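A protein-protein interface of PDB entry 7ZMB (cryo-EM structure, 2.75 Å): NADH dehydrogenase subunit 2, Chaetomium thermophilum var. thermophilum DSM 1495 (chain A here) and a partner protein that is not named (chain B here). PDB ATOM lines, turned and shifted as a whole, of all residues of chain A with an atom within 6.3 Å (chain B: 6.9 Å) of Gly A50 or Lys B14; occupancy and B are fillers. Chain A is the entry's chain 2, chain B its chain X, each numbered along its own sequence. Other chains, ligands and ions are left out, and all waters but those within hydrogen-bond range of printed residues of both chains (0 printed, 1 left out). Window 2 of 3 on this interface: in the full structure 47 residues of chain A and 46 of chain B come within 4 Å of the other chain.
O of Gly A52 sits at hydrogen-bond distance from NH2 of Arg B144, 3.1 Å away.
The backbone NH (N) of Gly A50 is in hydrogen-bond range of the side-chain hydroxyl (OG) of Ser A48 (3.1 Å).
N of Ile A51 is in hydrogen-bond range of O of Ile A60, 2.9 Å away.
Among the printed residues, merely in contact across the chains: Ile A51 with Arg B144, Gly A50 with Lys B14, Ile A51 with Val B16 and Phe A46 with Val B16.
Of chain A, only Gly A50 (3.5 Å) comes within 4 Å of Lys B14.
Printed residues of chain A within 4 Å of Val B16: Phe A46 (3.8 Å) and Ile A51 (3.6 Å).
Of the printed residues of chain B, Gly A52 touches Arg B144 (3.1 Å).
Of the printed residues of chain B, Ile A51 touches Val B16 and Arg B144.
Tyr B9 touches none of the printed residues of chain A.
Thr B15 touches none of the printed residues of chain A.
Of the 11 printed residues of chain B, 3 touch a printed residue of chain A.
Hydrophobic or aromatic side chains of chain B that line the printed part of chain A: Val B16.
Of the 11 printed residues of chain A, 4 touch a printed residue of chain B.
Hydrophobic or aromatic side chains of chain A that line the printed part of chain B: Phe A46 and Ile A51.
Among the printed residues, 5 pairs touch across the chains.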
ATOM      1  N   PHE A  46      -0.135  -5.021   0.189  1.00  0.00           N
ATOM      2  CA  PHE A  46       0.240  -4.803   1.608  1.00  0.00           C
ATOM      3  C   PHE A  46       0.180  -6.167   2.291  1.00  0.00           C
ATOM      4  O   PHE A  46      -0.643  -6.982   1.852  1.00  0.00           O
ATOM      5  CB  PHE A  46      -0.742  -3.830   2.271  1.00  0.00           C
ATOM      6  CG  PHE A  46      -2.120  -4.376   2.546  1.00  0.00           C
ATOM      7  CD1 PHE A  46      -3.101  -4.358   1.569  1.00  0.00           C
ATOM      8  CD2 PHE A  46      -2.444  -4.901   3.787  1.00  0.00           C
ATOM      9  CE1 PHE A  46      -4.365  -4.864   1.823  1.00  0.00           C
ATOM     10  CE2 PHE A  46      -3.709  -5.408   4.038  1.00  0.00           C
ATOM     11  CZ  PHE A  46      -4.667  -5.388   3.056  1.00  0.00           C
ATOM     12  N   SER A  48      -0.710  -7.850   5.860  1.00  0.00           N
ATOM     13  CA  SER A  48      -1.250  -7.430   7.176  1.00  0.00           C
ATOM     14  C   SER A  48      -2.320  -8.406   7.640  1.00  0.00           C
ATOM     15  O   SER A  48      -3.075  -8.886   6.784  1.00  0.00           O
ATOM     16  CB  SER A  48      -1.834  -6.036   7.085  1.00  0.00           C
ATOM     17  OG  SER A  48      -2.482  -5.668   8.295  1.00  0.00           O
ATOM     18  N   LYS A  49      -2.406  -8.659   8.938  1.00  0.00           N
ATOM     19  CA  LYS A  49      -3.556  -9.445   9.425  1.00  0.00           C
ATOM     20  C   LYS A  49      -4.823  -8.621   9.211  1.00  0.00           C
ATOM     21  O   LYS A  49      -5.828  -9.207   8.801  1.00  0.00           O
ATOM     22  CB  LYS A  49      -3.364  -9.795  10.902  1.00  0.00           C
ATOM     23  CG  LYS A  49      -2.415 -10.948  11.171  1.00  0.00           C
ATOM     24  CD  LYS A  49      -2.776 -11.722  12.411  1.00  0.00           C
ATOM     25  CE  LYS A  49      -1.719 -12.744  12.746  1.00  0.00           C
ATOM     26  NZ  LYS A  49      -0.379 -12.199  12.435  1.00  0.00           N
ATOM     27  N   GLY A  50      -4.791  -7.329   9.551  1.00  0.00           N
ATOM     28  CA  GLY A  50      -5.949  -6.451   9.320  1.00  0.00           C
ATOM     29  C   GLY A  50      -5.652  -4.979   9.521  1.00  0.00           C
ATOM     30  O   GLY A  50      -4.870  -4.658  10.417  1.00  0.00           O
ATOM     31  N   ILE A  51      -6.304  -4.115   8.749  1.00  0.00           N
ATOM     32  CA  ILE A  51      -6.152  -2.645   8.912  1.00  0.00           C
ATOM     33  C   ILE A  51      -7.530  -2.048   9.166  1.00  0.00           C
ATOM     34  O   ILE A  51      -8.365  -2.137   8.263  1.00  0.00           O
ATOM     35  CB  ILE A  51      -5.485  -2.023   7.673  1.00  0.00           C
ATOM     36  CG1 ILE A  51      -4.071  -2.556   7.437  1.00  0.00           C
ATOM     37  CG2 ILE A  51      -5.516  -0.505   7.719  1.00  0.00           C
ATOM     38  CD1 ILE A  51      -3.533  -2.217   6.072  1.00  0.00           C
ATOM     39  N   GLY A  52      -7.759  -1.490  10.357  1.00  0.00           N
ATOM     40  CA  GLY A  52      -8.999  -0.823  10.693  1.00  0.00           C
ATOM     41  C   GLY A  52      -9.296   0.354   9.788  1.00  0.00           C
ATOM     42  O   GLY A  52      -8.431   1.197   9.554  1.00  0.00           O
ATOM     43  N   HIS A  59     -12.776  -3.154   8.404  1.00  0.00           N
ATOM     44  CA  HIS A  59     -11.347  -3.564   8.327  1.00  0.00           C
ATOM     45  C   HIS A  59     -11.048  -4.105   6.937  1.00  0.00           C
ATOM     46  O   HIS A  59     -11.996  -4.466   6.229  1.00  0.00           O
ATOM     47  CB  HIS A  59     -10.961  -4.612   9.389  1.00  0.00           C
ATOM     48  CG  HIS A  59     -11.554  -5.961   9.152  1.00  0.00           C
ATOM     49  ND1 HIS A  59     -10.857  -6.970   8.523  1.00  0.00           N
ATOM     50  CD2 HIS A  59     -12.767  -6.470   9.451  1.00  0.00           C
ATOM     51  CE1 HIS A  59     -11.616  -8.041   8.443  1.00  0.00           C
ATOM     52  NE2 HIS A  59     -12.791  -7.762   9.004  1.00  0.00           N
ATOM     53  N   ILE A  60      -9.774  -4.124   6.558  1.00  0.00           N
ATOM     54  CA  ILE A  60      -9.370  -4.745   5.266  1.00  0.00           C
ATOM     55  C   ILE A  60      -8.269  -5.765   5.556  1.00  0.00           C
ATOM     56  O   ILE A  60      -7.395  -5.460   6.371  1.00  0.00           O
ATOM     57  CB  ILE A  60      -8.950  -3.697   4.217  1.00  0.00           C
ATOM     58  CG1 ILE A  60      -7.958  -2.684   4.792  1.00  0.00           C
ATOM     59  CG2 ILE A  60     -10.163  -3.013   3.611  1.00  0.00           C
ATOM     60  CD1 ILE A  60      -6.623  -2.696   4.101  1.00  0.00           C
ATOM     61  N   THR A  61      -8.344  -6.943   4.944  1.00  0.00           N
ATOM     62  CA  THR A  61      -7.330  -8.013   5.094  1.00  0.00           C
ATOM     63  C   THR A  61      -7.023  -8.497   3.675  1.00  0.00           C
ATOM     64  O   THR A  61      -7.820  -8.187   2.779  1.00  0.00           O
ATOM     65  CB  THR A  61      -7.854  -9.131   5.995  1.00  0.00           C
ATOM     66  OG1 THR A  61      -8.300  -8.536   7.212  1.00  0.00           O
ATOM     67  CG2 THR A  61      -6.802 -10.165   6.325  1.00  0.00           C
ATOM     68  N   GLU A 293     -12.538 -15.657  10.502  1.00  0.00           N
ATOM     69  CA  GLU A 293     -11.765 -14.714  11.340  1.00  0.00           C
ATOM     70  C   GLU A 293     -12.217 -14.821  12.798  1.00  0.00           C
ATOM     71  O   GLU A 293     -11.367 -14.728  13.689  1.00  0.00           O
ATOM     72  CB  GLU A 293     -11.839 -13.308  10.756  1.00  0.00           C
ATOM     73  CG  GLU A 293     -10.511 -12.801  10.230  1.00  0.00           C
ATOM     74  CD  GLU A 293     -10.515 -11.322   9.889  1.00  0.00           C
ATOM     75  OE1 GLU A 293      -9.845 -10.937   8.914  1.00  0.00           O
ATOM     76  OE2 GLU A 293     -11.184 -10.558  10.608  1.00  0.00           O
ATOM     77  N   TYR A 297      -9.683 -15.963  15.950  1.00  0.00           N
ATOM     78  CA  TYR A 297      -9.355 -15.019  17.055  1.00  0.00           C
ATOM     79  C   TYR A 297     -10.032 -15.401  18.379  1.00  0.00           C
ATOM     80  O   TYR A 297      -9.766 -14.726  19.386  1.00  0.00           O
ATOM     81  CB  TYR A 297      -9.568 -13.561  16.631  1.00  0.00           C
ATOM     82  CG  TYR A 297      -8.659 -13.031  15.554  1.00  0.00           C
ATOM     83  CD1 TYR A 297      -7.327 -12.761  15.808  1.00  0.00           C
ATOM     84  CD2 TYR A 297      -9.141 -12.754  14.287  1.00  0.00           C
ATOM     85  CE1 TYR A 297      -6.489 -12.258  14.828  1.00  0.00           C
ATOM     86  CE2 TYR A 297      -8.319 -12.253  13.294  1.00  0.00           C
ATOM     87  CZ  TYR A 297      -6.986 -12.005  13.563  1.00  0.00           C
ATOM     88  OH  TYR A 297      -6.172 -11.511  12.588  1.00  0.00           O
ATOM     89  N   TYR B   9       5.425  12.415  16.921  1.00  0.00           N
ATOM     90  CA  TYR B   9       4.439  11.319  16.759  1.00  0.00           C
ATOM     91  C   TYR B   9       3.398  11.484  17.861  1.00  0.00           C
ATOM     92  O   TYR B   9       3.516  10.802  18.872  1.00  0.00           O
ATOM     93  CB  TYR B   9       5.173   9.982  16.743  1.00  0.00           C
ATOM     94  CG  TYR B   9       4.394   8.780  16.282  1.00  0.00           C
ATOM     95  CD1 TYR B   9       4.397   8.390  14.954  1.00  0.00           C
ATOM     96  CD2 TYR B   9       3.694   8.002  17.187  1.00  0.00           C
ATOM     97  CE1 TYR B   9       3.699   7.272  14.531  1.00  0.00           C
ATOM     98  CE2 TYR B   9       2.993   6.883  16.781  1.00  0.00           C
ATOM     99  CZ  TYR B   9       2.995   6.518  15.450  1.00  0.00           C
ATOM    100  OH  TYR B   9       2.307   5.410  15.062  1.00  0.00           O
ATOM    101  N   PRO B  12      -1.254   7.570  18.013  1.00  0.00           N
ATOM    102  CA  PRO B  12      -0.911   6.196  17.660  1.00  0.00           C
ATOM    103  C   PRO B  12      -1.450   5.867  16.264  1.00  0.00           C
ATOM    104  O   PRO B  12      -2.586   6.155  15.998  1.00  0.00           O
ATOM    105  CB  PRO B  12      -1.550   5.401  18.805  1.00  0.00           C
ATOM    106  CG  PRO B  12      -2.757   6.211  19.210  1.00  0.00           C
ATOM    107  CD  PRO B  12      -2.341   7.648  18.992  1.00  0.00           C
ATOM    108  N   SER B  13      -0.623   5.274  15.405  1.00  0.00           N
ATOM    109  CA  SER B  13      -1.025   5.006  14.034  1.00  0.00           C
ATOM    110  C   SER B  13      -0.763   3.551  13.695  1.00  0.00           C
ATOM    111  O   SER B  13       0.104   2.903  14.280  1.00  0.00           O
ATOM    112  CB  SER B  13      -0.296   5.919  13.044  1.00  0.00           C
ATOM    113  OG  SER B  13       0.997   5.425  12.752  1.00  0.00           O
ATOM    114  N   LYS B  14      -1.499   3.043  12.707  1.00  0.00           N
ATOM    115  CA  LYS B  14      -1.343   1.629  12.278  1.00  0.00           C
ATOM    116  C   LYS B  14      -0.101   1.493  11.404  1.00  0.00           C
ATOM    117  O   LYS B  14       0.071   2.320  10.500  1.00  0.00           O
ATOM    118  CB  LYS B  14      -2.583   1.147  11.525  1.00  0.00           C
ATOM    119  CG  LYS B  14      -2.555  -0.299  11.050  1.00  0.00           C
ATOM    120  CD  LYS B  14      -2.404  -1.299  12.171  1.00  0.00           C
ATOM    121  CE  LYS B  14      -2.251  -2.723  11.686  1.00  0.00           C
ATOM    122  NZ  LYS B  14      -2.101  -3.665  12.821  1.00  0.00           N
ATOM    123  N   THR B  15       0.741   0.500  11.709  1.00  0.00           N
ATOM    124  CA  THR B  15       1.940   0.218  10.884  1.00  0.00           C
ATOM    125  C   THR B  15       1.580  -0.929   9.942  1.00  0.00           C
ATOM    126  O   THR B  15       1.039  -1.937  10.419  1.00  0.00           O
ATOM    127  CB  THR B  15       3.165  -0.054  11.765  1.00  0.00           C
ATOM    128  OG1 THR B  15       3.659   1.216  12.189  1.00  0.00           O
ATOM    129  CG2 THR B  15       4.262  -0.810  11.051  1.00  0.00           C
ATOM    130  N   VAL B  16       1.883  -0.779   8.659  1.00  0.00           N
ATOM    131  CA  VAL B  16       1.543  -1.828   7.661  1.00  0.00           C
ATOM    132  C   VAL B  16       2.852  -2.308   7.034  1.00  0.00           C
ATOM    133  O   VAL B  16       3.759  -1.476   6.858  1.00  0.00           O
ATOM    134  CB  VAL B  16       0.550  -1.300   6.607  1.00  0.00           C
ATOM    135  CG1 VAL B  16       0.013  -2.414   5.725  1.00  0.00           C
ATOM    136  CG2 VAL B  16      -0.590  -0.524   7.245  1.00  0.00           C
ATOM    137  N   LEU B  22       6.662   4.958   3.620  1.00  0.00           N
ATOM    138  CA  LEU B  22       5.360   5.618   3.871  1.00  0.00           C
ATOM    139  C   LEU B  22       5.567   7.132   3.910  1.00  0.00           C
ATOM    140  O   LEU B  22       6.431   7.587   4.667  1.00  0.00           O
ATOM    141  CB  LEU B  22       4.755   5.101   5.179  1.00  0.00           C
ATOM    142  CG  LEU B  22       3.533   5.870   5.685  1.00  0.00           C
ATOM    143  CD1 LEU B  22       2.319   5.630   4.800  1.00  0.00           C
ATOM    144  CD2 LEU B  22       3.216   5.525   7.131  1.00  0.00           C
ATOM    145  N   ASN B  25      -0.358   8.480   5.253  1.00  0.00           N
ATOM    146  CA  ASN B  25      -1.491   7.518   5.250  1.00  0.00           C
ATOM    147  C   ASN B  25      -2.827   8.232   5.014  1.00  0.00           C
ATOM    148  O   ASN B  25      -3.803   7.538   4.716  1.00  0.00           O
ATOM    149  CB  ASN B  25      -1.463   6.602   6.477  1.00  0.00           C
ATOM    150  CG  ASN B  25      -1.742   7.256   7.813  1.00  0.00           C
ATOM    151  OD1 ASN B  25      -2.354   8.317   7.902  1.00  0.00           O
ATOM    152  ND2 ASN B  25      -1.318   6.597   8.875  1.00  0.00           N
ATOM    153  N   ARG B 144      -7.803   7.499   6.889  1.00  0.00           N
ATOM    154  CA  ARG B 144      -6.448   7.001   6.683  1.00  0.00           C
ATOM    155  C   ARG B 144      -6.501   5.596   6.088  1.00  0.00           C
ATOM    156  O   ARG B 144      -7.284   4.749   6.526  1.00  0.00           O
ATOM    157  CB  ARG B 144      -5.627   7.046   7.984  1.00  0.00           C
ATOM    158  CG  ARG B 144      -6.160   6.260   9.157  1.00  0.00           C
ATOM    159  CD  ARG B 144      -5.680   4.827   9.147  1.00  0.00           C
ATOM    160  NE  ARG B 144      -6.086   4.118  10.347  1.00  0.00           N
ATOM    161  CZ  ARG B 144      -5.918   2.820  10.529  1.00  0.00           C
ATOM    162  NH1 ARG B 144      -5.369   2.104   9.574  1.00  0.00           N
ATOM    163  NH2 ARG B 144      -6.331   2.235  11.638  1.00  0.00           N
ATOM    164  N   TYR B 145      -5.694   5.371   5.050  1.00  0.00           N
ATOM    165  CA  TYR B 145      -5.664   4.116   4.294  1.00  0.00           C
ATOM    166  C   TYR B 145      -7.007   3.792   3.651  1.00  0.00           C
ATOM    167  O   TYR B 145      -7.298   2.633   3.364  1.00  0.00           O
ATOM    168  CB  TYR B 145      -5.211   2.942   5.166  1.00  0.00           C
ATOM    169  CG  TYR B 145      -3.775   3.015   5.595  1.00  0.00           C
ATOM    170  CD1 TYR B 145      -2.762   3.172   4.667  1.00  0.00           C
ATOM    171  CD2 TYR B 145      -3.432   2.912   6.931  1.00  0.00           C
ATOM    172  CE1 TYR B 145      -1.454   3.235   5.056  1.00  0.00           C
ATOM    173  CE2 TYR B 145      -2.126   2.976   7.331  1.00  0.00           C
ATOM    174  CZ  TYR B 145      -1.141   3.140   6.392  1.00  0.00           C
ATOM    175  OH  TYR B 145       0.165   3.199   6.798  1.00  0.00           O
ATOM    176  N   GLY B 165       0.393   9.809  10.287  1.00  0.00           N
ATOM    177  CA  GLY B 165       1.091   8.521  10.476  1.00  0.00           C
ATOM    178  C   GLY B 165       2.606   8.554  10.353  1.00  0.00           C
ATOM    179  O   GLY B 165       3.209   7.492  10.533  1.00  0.00           O
